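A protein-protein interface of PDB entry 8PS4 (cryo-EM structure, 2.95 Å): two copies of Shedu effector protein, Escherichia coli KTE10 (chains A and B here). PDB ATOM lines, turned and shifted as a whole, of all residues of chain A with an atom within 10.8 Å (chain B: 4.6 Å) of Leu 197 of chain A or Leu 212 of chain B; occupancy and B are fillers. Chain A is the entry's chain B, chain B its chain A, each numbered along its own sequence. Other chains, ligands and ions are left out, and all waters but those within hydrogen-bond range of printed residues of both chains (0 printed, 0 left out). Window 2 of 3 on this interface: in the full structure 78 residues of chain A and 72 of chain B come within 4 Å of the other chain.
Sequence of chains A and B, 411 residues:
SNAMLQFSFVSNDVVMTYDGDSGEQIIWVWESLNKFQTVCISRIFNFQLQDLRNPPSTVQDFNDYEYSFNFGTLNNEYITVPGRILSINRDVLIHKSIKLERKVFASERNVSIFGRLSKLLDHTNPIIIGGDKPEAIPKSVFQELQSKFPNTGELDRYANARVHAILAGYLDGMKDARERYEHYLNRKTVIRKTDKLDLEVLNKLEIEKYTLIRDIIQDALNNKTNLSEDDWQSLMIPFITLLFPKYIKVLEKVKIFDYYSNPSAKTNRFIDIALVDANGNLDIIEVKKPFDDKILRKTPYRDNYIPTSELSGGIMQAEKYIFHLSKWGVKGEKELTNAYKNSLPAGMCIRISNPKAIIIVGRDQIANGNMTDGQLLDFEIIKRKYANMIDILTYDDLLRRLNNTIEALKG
Leu 205 of chain A touches its own counterpart, Leu 205 of chain B. Position printed for both chains: 205.
Among the printed residues, merely in contact across the chains: Tyr 184 of chain A with Leu 205 of chain B (3.5 Å), Leu 197 of chain A with Glu 208 of chain B (3.5 Å), Leu 197 of chain A with Leu 212 of chain B (3.9 Å), Leu 202 of chain A with Lys 209 of chain B (3.8 Å), Leu 202 of chain A with Leu 212 of chain B (3.8 Å) and Leu 205 of chain A with Leu 205 of chain B (3.3 Å).
Along chain B the printed residues that touch a printed residue of chain A span positions 205 to 212. Of the 20 printed residues of chain A, 6 touch a printed residue of chain B. Hydrophobic or aromatic side chains of chain A within 4 Å of the printed part of chain B: Tyr 184, Leu 197, Leu 202 and Leu 205. Among the printed residues, 8 pairs touch across the chains. Among the printed residues, Asp or Glu carboxylates within 4 Å of a Lys or Arg side-chain nitrogen of the other chain: Arg 192 of chain A with Glu 208 of chain B (2.9 Å) and Glu 206 of chain A with Lys 209 of chain B (3.2 Å).
O of Glu 208 of chain B lies within hydrogen-bond range of OG1 of Thr 211 of chain B (3.0 Å). The side-chain carboxylate of Asp 195 of chain A is in salt-bridge range of the guanidinium group of Arg 192 of chain A (3.4 Å).
Thr 189 of chain A touches none of the printed residues of chain B. Printed residues of chain B within 4 Å of Arg 192 of chain A: Glu 208 (2.9 Å). Of chain B, only Glu 208 (3.5 Å) and Leu 212 (3.9 Å) come within 4 Å of Leu 197 of chain A. Of the printed residues of chain B, Leu 205 of chain A touches Leu 205. Of the printed residues of chain A, Leu 205 of chain B touches Tyr 184 (3.5 Å) and Leu 205 (3.3 Å). Of the printed residues of chain A, Glu 208 of chain B touches Arg 192 (2.9 Å) and Leu 197 (3.5 Å). Thr 211 of chain B touches none of the printed residues of chain A. Of chain A, only Leu 197 (3.9 Å) and Leu 202 (3.8 Å) come within 4 Å of Leu 212 of chain B. No residue of chain A comes within 4 Å of Ile 213 of chain B. Asp 215 of chain B touches none of the printed residues of chain A. No residue of chain A comes within 4 Å of Ile 216 of chain B. The nearest residue of chain A that does not touch Leu 212 of chain B is Leu 199 of chain A (5.0 Å). The nearest printed residue of chain A that does not touch Leu 205 of chain B is Arg 192 of chain A (4.1 Å).
The side-chain carboxylate of Glu 208 of chain B is in salt-bridge range of the guanidinium group of Arg 192 of chain A, 2.9 Å away. The side-chain amino group (NZ) of Lys 209 of chain B is in salt-bridge range of the side-chain carboxylate (OE2) of Glu 206 of chain A (3.2 Å).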
ATOM      1  N   TYR A 184     -11.422  11.133  12.370  1.00  0.00           N
ATOM      2  CA  TYR A 184     -11.266  10.134  11.279  1.00  0.00           C
ATOM      3  C   TYR A 184     -10.243  10.654  10.269  1.00  0.00           C
ATOM      4  O   TYR A 184      -9.397   9.864   9.826  1.00  0.00           O
ATOM      5  CB  TYR A 184     -12.603   9.859  10.586  1.00  0.00           C
ATOM      6  CG  TYR A 184     -12.486   9.293   9.193  1.00  0.00           C
ATOM      7  CD1 TYR A 184     -12.148   7.966   8.988  1.00  0.00           C
ATOM      8  CD2 TYR A 184     -12.711  10.081   8.077  1.00  0.00           C
ATOM      9  CE1 TYR A 184     -12.032   7.437   7.713  1.00  0.00           C
ATOM     10  CE2 TYR A 184     -12.598   9.570   6.795  1.00  0.00           C
ATOM     11  CZ  TYR A 184     -12.259   8.242   6.612  1.00  0.00           C
ATOM     12  OH  TYR A 184     -12.150   7.727   5.353  1.00  0.00           O
ATOM     13  N   LYS A 188      -6.953   8.805   9.127  1.00  0.00           N
ATOM     14  CA  LYS A 188      -6.809   8.407   7.702  1.00  0.00           C
ATOM     15  C   LYS A 188      -5.444   8.876   7.193  1.00  0.00           C
ATOM     16  O   LYS A 188      -4.775   8.091   6.503  1.00  0.00           O
ATOM     17  CB  LYS A 188      -7.950   9.007   6.873  1.00  0.00           C
ATOM     18  CG  LYS A 188      -7.751   9.000   5.364  1.00  0.00           C
ATOM     19  CD  LYS A 188      -8.466  10.136   4.668  1.00  0.00           C
ATOM     20  CE  LYS A 188      -7.881  11.492   5.000  1.00  0.00           C
ATOM     21  NZ  LYS A 188      -6.451  11.580   4.626  1.00  0.00           N
ATOM     22  N   THR A 189      -5.038  10.096   7.556  1.00  0.00           N
ATOM     23  CA  THR A 189      -3.734  10.639   7.094  1.00  0.00           C
ATOM     24  C   THR A 189      -2.598   9.770   7.643  1.00  0.00           C
ATOM     25  O   THR A 189      -1.664   9.467   6.874  1.00  0.00           O
ATOM     26  CB  THR A 189      -3.572  12.106   7.506  1.00  0.00           C
ATOM     27  OG1 THR A 189      -4.786  12.787   7.189  1.00  0.00           O
ATOM     28  CG2 THR A 189      -2.413  12.789   6.816  1.00  0.00           C
ATOM     29  N   VAL A 190      -2.683   9.380   8.918  1.00  0.00           N
ATOM     30  CA  VAL A 190      -1.608   8.552   9.544  1.00  0.00           C
ATOM     31  C   VAL A 190      -1.542   7.194   8.835  1.00  0.00           C
ATOM     32  O   VAL A 190      -0.425   6.752   8.517  1.00  0.00           O
ATOM     33  CB  VAL A 190      -1.847   8.387  11.057  1.00  0.00           C
ATOM     34  CG1 VAL A 190      -0.935   7.337  11.671  1.00  0.00           C
ATOM     35  CG2 VAL A 190      -1.712   9.710  11.796  1.00  0.00           C
ATOM     36  N   ILE A 191      -2.695   6.567   8.590  1.00  0.00           N
ATOM     37  CA  ILE A 191      -2.733   5.228   7.927  1.00  0.00           C
ATOM     38  C   ILE A 191      -2.249   5.348   6.478  1.00  0.00           C
ATOM     39  O   ILE A 191      -1.456   4.486   6.048  1.00  0.00           O
ATOM     40  CB  ILE A 191      -4.146   4.620   8.028  1.00  0.00           C
ATOM     41  CG1 ILE A 191      -4.474   4.216   9.466  1.00  0.00           C
ATOM     42  CG2 ILE A 191      -4.314   3.455   7.066  1.00  0.00           C
ATOM     43  CD1 ILE A 191      -5.855   3.642   9.638  1.00  0.00           C
ATOM     44  N   ARG A 192      -2.674   6.396   5.767  1.00  0.00           N
ATOM     45  CA  ARG A 192      -2.324   6.536   4.329  1.00  0.00           C
ATOM     46  C   ARG A 192      -1.078   7.410   4.182  1.00  0.00           C
ATOM     47  O   ARG A 192      -1.169   8.444   3.492  1.00  0.00           O
ATOM     48  CB  ARG A 192      -3.492   7.161   3.561  1.00  0.00           C
ATOM     49  CG  ARG A 192      -4.065   6.274   2.468  1.00  0.00           C
ATOM     50  CD  ARG A 192      -5.132   7.006   1.680  1.00  0.00           C
ATOM     51  NE  ARG A 192      -4.614   8.206   1.042  1.00  0.00           N
ATOM     52  CZ  ARG A 192      -4.379   8.322  -0.260  1.00  0.00           C
ATOM     53  NH1 ARG A 192      -4.620   7.305  -1.067  1.00  0.00           N
ATOM     54  NH2 ARG A 192      -3.907   9.455  -0.748  1.00  0.00           N
ATOM     55  N   LYS A 193       0.034   7.013   4.807  1.00  0.00           N
ATOM     56  CA  LYS A 193       1.303   7.769   4.633  1.00  0.00           C
ATOM     57  C   LYS A 193       1.611   7.860   3.136  1.00  0.00           C
ATOM     58  O   LYS A 193       2.080   8.926   2.693  1.00  0.00           O
ATOM     59  CB  LYS A 193       2.438   7.073   5.387  1.00  0.00           C
ATOM     60  CG  LYS A 193       2.320   7.106   6.905  1.00  0.00           C
ATOM     61  CD  LYS A 193       3.183   6.074   7.596  1.00  0.00           C
ATOM     62  CE  LYS A 193       2.735   4.654   7.323  1.00  0.00           C
ATOM     63  NZ  LYS A 193       1.361   4.408   7.821  1.00  0.00           N
ATOM     64  N   THR A 194       1.351   6.779   2.393  1.00  0.00           N
ATOM     65  CA  THR A 194       1.649   6.747   0.937  1.00  0.00           C
ATOM     66  C   THR A 194       0.347   6.865   0.143  1.00  0.00           C
ATOM     67  O   THR A 194      -0.663   6.274   0.575  1.00  0.00           O
ATOM     68  CB  THR A 194       2.398   5.464   0.553  1.00  0.00           C
ATOM     69  OG1 THR A 194       1.517   4.357   0.746  1.00  0.00           O
ATOM     70  CG2 THR A 194       3.665   5.258   1.353  1.00  0.00           C
ATOM     71  N   ASP A 195       0.372   7.609  -0.966  1.00  0.00           N
ATOM     72  CA  ASP A 195      -0.827   7.759  -1.835  1.00  0.00           C
ATOM     73  C   ASP A 195      -1.215   6.385  -2.392  1.00  0.00           C
ATOM     74  O   ASP A 195      -2.427   6.124  -2.525  1.00  0.00           O
ATOM     75  CB  ASP A 195      -0.596   8.798  -2.933  1.00  0.00           C
ATOM     76  CG  ASP A 195      -0.432  10.207  -2.391  1.00  0.00           C
ATOM     77  OD1 ASP A 195      -0.666  10.400  -1.182  1.00  0.00           O
ATOM     78  OD2 ASP A 195      -0.068  11.099  -3.183  1.00  0.00           O
ATOM     79  N   LYS A 196      -0.222   5.547  -2.707  1.00  0.00           N
ATOM     80  CA  LYS A 196      -0.497   4.199  -3.272  1.00  0.00           C
ATOM     81  C   LYS A 196      -1.342   3.409  -2.268  1.00  0.00           C
ATOM     82  O   LYS A 196      -1.058   3.502  -1.057  1.00  0.00           O
ATOM     83  CB  LYS A 196       0.821   3.471  -3.547  1.00  0.00           C
ATOM     84  CG  LYS A 196       1.846   4.267  -4.343  1.00  0.00           C
ATOM     85  CD  LYS A 196       3.159   3.537  -4.526  1.00  0.00           C
ATOM     86  CE  LYS A 196       4.182   4.346  -5.294  1.00  0.00           C
ATOM     87  NZ  LYS A 196       5.454   3.603  -5.461  1.00  0.00           N
ATOM     88  N   LEU A 197      -2.329   2.652  -2.755  1.00  0.00           N
ATOM     89  CA  LEU A 197      -3.255   1.937  -1.836  1.00  0.00           C
ATOM     90  C   LEU A 197      -2.965   0.435  -1.837  1.00  0.00           C
ATOM     91  O   LEU A 197      -2.806  -0.137  -2.933  1.00  0.00           O
ATOM     92  CB  LEU A 197      -4.701   2.215  -2.256  1.00  0.00           C
ATOM     93  CG  LEU A 197      -5.274   3.544  -1.771  1.00  0.00           C
ATOM     94  CD1 LEU A 197      -6.757   3.630  -2.087  1.00  0.00           C
ATOM     95  CD2 LEU A 197      -5.045   3.711  -0.277  1.00  0.00           C
ATOM     96  N   ASP A 198      -2.887  -0.172  -0.649  1.00  0.00           N
ATOM     97  CA  ASP A 198      -2.682  -1.642  -0.542  1.00  0.00           C
ATOM     98  C   ASP A 198      -3.965  -2.233   0.052  1.00  0.00           C
ATOM     99  O   ASP A 198      -4.741  -1.460   0.636  1.00  0.00           O
ATOM    100  CB  ASP A 198      -1.453  -1.961   0.313  1.00  0.00           C
ATOM    101  CG  ASP A 198      -1.049  -3.426   0.296  1.00  0.00           C
ATOM    102  OD1 ASP A 198      -1.318  -4.097  -0.719  1.00  0.00           O
ATOM    103  OD2 ASP A 198      -0.477  -3.886   1.304  1.00  0.00           O
ATOM    104  N   LEU A 199      -4.171  -3.544  -0.090  1.00  0.00           N
ATOM    105  CA  LEU A 199      -5.377  -4.201   0.480  1.00  0.00           C
ATOM    106  C   LEU A 199      -5.358  -4.052   2.006  1.00  0.00           C
ATOM    107  O   LEU A 199      -6.425  -3.768   2.579  1.00  0.00           O
ATOM    108  CB  LEU A 199      -5.387  -5.674   0.065  1.00  0.00           C
ATOM    109  CG  LEU A 199      -5.563  -5.925  -1.432  1.00  0.00           C
ATOM    110  CD1 LEU A 199      -5.451  -7.408  -1.751  1.00  0.00           C
ATOM    111  CD2 LEU A 199      -6.895  -5.374  -1.919  1.00  0.00           C
ATOM    112  N   GLU A 200      -4.186  -4.222   2.629  1.00  0.00           N
ATOM    113  CA  GLU A 200      -4.067  -4.048   4.101  1.00  0.00           C
ATOM    114  C   GLU A 200      -4.392  -2.596   4.467  1.00  0.00           C
ATOM    115  O   GLU A 200      -5.137  -2.385   5.444  1.00  0.00           O
ATOM    116  CB  GLU A 200      -2.650  -4.403   4.555  1.00  0.00           C
ATOM    117  CG  GLU A 200      -2.413  -4.168   6.037  1.00  0.00           C
ATOM    118  CD  GLU A 200      -0.962  -4.268   6.469  1.00  0.00           C
ATOM    119  OE1 GLU A 200      -0.109  -4.566   5.609  1.00  0.00           O
ATOM    120  OE2 GLU A 200      -0.686  -4.044   7.665  1.00  0.00           O
ATOM    121  N   VAL A 201      -3.877  -1.641   3.686  1.00  0.00           N
ATOM    122  CA  VAL A 201      -4.133  -0.195   3.962  1.00  0.00           C
ATOM    123  C   VAL A 201      -5.635   0.065   3.820  1.00  0.00           C
ATOM    124  O   VAL A 201      -6.195   0.762   4.686  1.00  0.00           O
ATOM    125  CB  VAL A 201      -3.300   0.713   3.036  1.00  0.00           C
ATOM    126  CG1 VAL A 201      -3.614   2.187   3.245  1.00  0.00           C
ATOM    127  CG2 VAL A 201      -1.810   0.459   3.199  1.00  0.00           C
ATOM    128  N   LEU A 202      -6.265  -0.523   2.799  1.00  0.00           N
ATOM    129  CA  LEU A 202      -7.719  -0.316   2.568  1.00  0.00           C
ATOM    130  C   LEU A 202      -8.501  -0.853   3.769  1.00  0.00           C
ATOM    131  O   LEU A 202      -9.451  -0.178   4.193  1.00  0.00           O
ATOM    132  CB  LEU A 202      -8.136  -1.039   1.284  1.00  0.00           C
ATOM    133  CG  LEU A 202      -7.819  -0.298  -0.012  1.00  0.00           C
ATOM    134  CD1 LEU A 202      -8.291  -1.097  -1.216  1.00  0.00           C
ATOM    135  CD2 LEU A 202      -8.454   1.082  -0.004  1.00  0.00           C
ATOM    136  N   ASN A 203      -8.101  -2.014   4.295  1.00  0.00           N
ATOM    137  CA  ASN A 203      -8.820  -2.625   5.445  1.00  0.00           C
ATOM    138  C   ASN A 203      -8.717  -1.698   6.659  1.00  0.00           C
ATOM    139  O   ASN A 203      -9.740  -1.515   7.339  1.00  0.00           O
ATOM    140  CB  ASN A 203      -8.301  -4.030   5.759  1.00  0.00           C
ATOM    141  CG  ASN A 203      -8.578  -5.019   4.646  1.00  0.00           C
ATOM    142  OD1 ASN A 203      -9.337  -4.726   3.725  1.00  0.00           O
ATOM    143  ND2 ASN A 203      -7.969  -6.190   4.723  1.00  0.00           N
ATOM    144  N   LYS A 204      -7.535  -1.124   6.901  1.00  0.00           N
ATOM    145  CA  LYS A 204      -7.346  -0.188   8.043  1.00  0.00           C
ATOM    146  C   LYS A 204      -8.218   1.055   7.839  1.00  0.00           C
ATOM    147  O   LYS A 204      -8.835   1.509   8.823  1.00  0.00           O
ATOM    148  CB  LYS A 204      -5.864   0.170   8.199  1.00  0.00           C
ATOM    149  CG  LYS A 204      -4.964  -0.979   8.630  1.00  0.00           C
ATOM    150  CD  LYS A 204      -3.510  -0.588   8.769  1.00  0.00           C
ATOM    151  CE  LYS A 204      -2.880  -0.167   7.459  1.00  0.00           C
ATOM    152  NZ  LYS A 204      -1.465   0.238   7.632  1.00  0.00           N
ATOM    153  N   LEU A 205      -8.274   1.574   6.608  1.00  0.00           N
ATOM    154  CA  LEU A 205      -9.132   2.752   6.303  1.00  0.00           C
ATOM    155  C   LEU A 205     -10.601   2.375   6.520  1.00  0.00           C
ATOM    156  O   LEU A 205     -11.354   3.222   7.035  1.00  0.00           O
ATOM    157  CB  LEU A 205      -8.878   3.200   4.861  1.00  0.00           C
ATOM    158  CG  LEU A 205      -7.483   3.761   4.590  1.00  0.00           C
ATOM    159  CD1 LEU A 205      -7.236   3.905   3.096  1.00  0.00           C
ATOM    160  CD2 LEU A 205      -7.281   5.091   5.301  1.00  0.00           C
ATOM    161  N   GLU A 206     -10.986   1.154   6.136  1.00  0.00           N
ATOM    162  CA  GLU A 206     -12.387   0.687   6.322  1.00  0.00           C
ATOM    163  C   GLU A 206     -12.714   0.656   7.818  1.00  0.00           C
ATOM    164  O   GLU A 206     -13.824   1.071   8.181  1.00  0.00           O
ATOM    165  CB  GLU A 206     -12.596  -0.691   5.688  1.00  0.00           C
ATOM    166  CG  GLU A 206     -12.638  -0.659   4.172  1.00  0.00           C
ATOM    167  CD  GLU A 206     -13.803   0.119   3.586  1.00  0.00           C
ATOM    168  OE1 GLU A 206     -14.959  -0.259   3.856  1.00  0.00           O
ATOM    169  OE2 GLU A 206     -13.550   1.106   2.867  1.00  0.00           O
ATOM    170  N   LEU B 205     -11.971   8.440  -0.889  1.00  0.00           N
ATOM    171  CA  LEU B 205     -11.269   7.182  -0.521  1.00  0.00           C
ATOM    172  C   LEU B 205     -12.085   5.975  -0.993  1.00  0.00           C
ATOM    173  O   LEU B 205     -11.470   4.987  -1.425  1.00  0.00           O
ATOM    174  CB  LEU B 205     -11.013   7.148   0.987  1.00  0.00           C
ATOM    175  CG  LEU B 205     -10.359   5.862   1.486  1.00  0.00           C
ATOM    176  CD1 LEU B 205      -8.979   5.698   0.873  1.00  0.00           C
ATOM    177  CD2 LEU B 205     -10.258   5.866   3.005  1.00  0.00           C
ATOM    178  N   GLU B 208     -11.387   5.602  -4.523  1.00  0.00           N
ATOM    179  CA  GLU B 208     -10.013   5.062  -4.696  1.00  0.00           C
ATOM    180  C   GLU B 208     -10.026   3.551  -4.448  1.00  0.00           C
ATOM    181  O   GLU B 208      -9.266   2.840  -5.126  1.00  0.00           O
ATOM    182  CB  GLU B 208      -9.040   5.760  -3.747  1.00  0.00           C
ATOM    183  CG  GLU B 208      -8.709   7.184  -4.145  1.00  0.00           C
ATOM    184  CD  GLU B 208      -8.185   8.038  -3.004  1.00  0.00           C
ATOM    185  OE1 GLU B 208      -7.225   7.603  -2.338  1.00  0.00           O
ATOM    186  OE2 GLU B 208      -8.739   9.132  -2.781  1.00  0.00           O
ATOM    187  N   LYS B 209     -10.859   3.088  -3.510  1.00  0.00           N
ATOM    188  CA  LYS B 209     -10.956   1.633  -3.223  1.00  0.00           C
ATOM    189  C   LYS B 209     -11.676   0.934  -4.377  1.00  0.00           C
ATOM    190  O   LYS B 209     -11.174  -0.105  -4.843  1.00  0.00           O
ATOM    191  CB  LYS B 209     -11.755   1.404  -1.935  1.00  0.00           C
ATOM    192  CG  LYS B 209     -12.075  -0.052  -1.623  1.00  0.00           C
ATOM    193  CD  LYS B 209     -13.034  -0.225  -0.468  1.00  0.00           C
ATOM    194  CE  LYS B 209     -14.382   0.411  -0.725  1.00  0.00           C
ATOM    195  NZ  LYS B 209     -15.343   0.117   0.364  1.00  0.00           N
ATOM    196  N   TYR B 210     -12.793   1.504  -4.838  1.00  0.00           N
ATOM    197  CA  TYR B 210     -13.589   0.861  -5.915  1.00  0.00           C
ATOM    198  C   TYR B 210     -12.799   0.834  -7.230  1.00  0.00           C
ATOM    199  O   TYR B 210     -12.857  -0.191  -7.932  1.00  0.00           O
ATOM    200  CB  TYR B 210     -14.989   1.471  -6.004  1.00  0.00           C
ATOM    201  CG  TYR B 210     -15.895   1.085  -4.862  1.00  0.00           C
ATOM    202  CD1 TYR B 210     -16.145  -0.245  -4.569  1.00  0.00           C
ATOM    203  CD2 TYR B 210     -16.503   2.045  -4.072  1.00  0.00           C
ATOM    204  CE1 TYR B 210     -16.973  -0.613  -3.522  1.00  0.00           C
ATOM    205  CE2 TYR B 210     -17.332   1.696  -3.018  1.00  0.00           C
ATOM    206  CZ  TYR B 210     -17.571   0.361  -2.744  1.00  0.00           C
ATOM    207  OH  TYR B 210     -18.388   0.009  -1.709  1.00  0.00           O
ATOM    208  N   THR B 211     -12.115   1.936  -7.559  1.00  0.00           N
ATOM    209  CA  THR B 211     -11.314   1.992  -8.811  1.00  0.00           C
ATOM    210  C   THR B 211     -10.233   0.913  -8.755  1.00  0.00           C
ATOM    211  O   THR B 211     -10.044   0.230  -9.771  1.00  0.00           O
ATOM    212  CB  THR B 211     -10.704   3.379  -9.062  1.00  0.00           C
ATOM    213  OG1 THR B 211      -9.969   3.778  -7.905  1.00  0.00           O
ATOM    214  CG2 THR B 211     -11.732   4.432  -9.411  1.00  0.00           C
ATOM    215  N   LEU B 212      -9.561   0.764  -7.609  1.00  0.00           N
ATOM    216  CA  LEU B 212      -8.444  -0.211  -7.517  1.00  0.00           C
ATOM    217  C   LEU B 212      -8.983  -1.626  -7.759  1.00  0.00           C
ATOM    218  O   LEU B 212      -8.380  -2.352  -8.569  1.00  0.00           O
ATOM    219  CB  LEU B 212      -7.813  -0.104  -6.126  1.00  0.00           C
ATOM    220  CG  LEU B 212      -6.638  -1.045  -5.860  1.00  0.00           C
ATOM    221  CD1 LEU B 212      -5.439  -0.667  -6.716  1.00  0.00           C
ATOM    222  CD2 LEU B 212      -6.262  -1.039  -4.388  1.00  0.00           C
ATOM    223  N   ILE B 213     -10.107  -1.975  -7.124  1.00  0.00           N
ATOM    224  CA  ILE B 213     -10.698  -3.335  -7.293  1.00  0.00           C
ATOM    225  C   ILE B 213     -11.120  -3.500  -8.755  1.00  0.00           C
ATOM    226  O   ILE B 213     -10.796  -4.545  -9.348  1.00  0.00           O
ATOM    227  CB  ILE B 213     -11.893  -3.533  -6.338  1.00  0.00           C
ATOM    228  CG1 ILE B 213     -11.498  -3.326  -4.875  1.00  0.00           C
ATOM    229  CG2 ILE B 213     -12.542  -4.891  -6.552  1.00  0.00           C
ATOM    230  CD1 ILE B 213     -12.677  -3.284  -3.933  1.00  0.00           C
ATOM    231  N   ARG B 214     -11.764  -2.476  -9.323  1.00  0.00           N
ATOM    232  CA  ARG B 214     -12.263  -2.566 -10.719  1.00  0.00           C
ATOM    233  C   ARG B 214     -11.074  -2.736 -11.666  1.00  0.00           C
ATOM    234  O   ARG B 214     -11.155  -3.594 -12.562  1.00  0.00           O
ATOM    235  CB  ARG B 214     -13.045  -1.297 -11.067  1.00  0.00           C
ATOM    236  CG  ARG B 214     -13.558  -1.241 -12.498  1.00  0.00           C
ATOM    237  CD  ARG B 214     -13.804   0.199 -12.896  1.00  0.00           C
ATOM    238  NE  ARG B 214     -12.601   1.001 -12.726  1.00  0.00           N
ATOM    239  CZ  ARG B 214     -12.532   2.307 -12.945  1.00  0.00           C
ATOM    240  NH1 ARG B 214     -13.604   2.970 -13.344  1.00  0.00           N
ATOM    241  NH2 ARG B 214     -11.391   2.949 -12.764  1.00  0.00           N
ATOM    242  N   ASP B 215     -10.001  -1.970 -11.445  1.00  0.00           N
ATOM    243  CA  ASP B 215      -8.820  -2.031 -12.345  1.00  0.00           C
ATOM    244  C   ASP B 215      -8.197  -3.427 -12.273  1.00  0.00           C
ATOM    245  O   ASP B 215      -7.836  -3.957 -13.334  1.00  0.00           O
ATOM    246  CB  ASP B 215      -7.809  -0.929 -12.022  1.00  0.00           C
ATOM    247  CG  ASP B 215      -8.313   0.462 -12.364  1.00  0.00           C
ATOM    248  OD1 ASP B 215      -9.390   0.558 -12.986  1.00  0.00           O
ATOM    249  OD2 ASP B 215      -7.628   1.438 -12.001  1.00  0.00           O
ATOM    250  N   ILE B 216      -8.051  -3.991 -11.070  1.00  0.00           N
ATOM    251  CA  ILE B 216      -7.360  -5.310 -10.937  1.00  0.00           C
ATOM    252  C   ILE B 216      -8.196  -6.393 -11.630  1.00  0.00           C
ATOM    253  O   ILE B 216      -7.618  -7.169 -12.414  1.00  0.00           O
ATOM    254  CB  ILE B 216      -7.058  -5.645  -9.463  1.00  0.00           C
ATOM    255  CG1 ILE B 216      -6.123  -4.606  -8.838  1.00  0.00           C
ATOM    256  CG2 ILE B 216      -6.486  -7.049  -9.337  1.00  0.00           C
ATOM    257  CD1 ILE B 216      -5.813  -4.852  -7.381  1.00  0.00           C
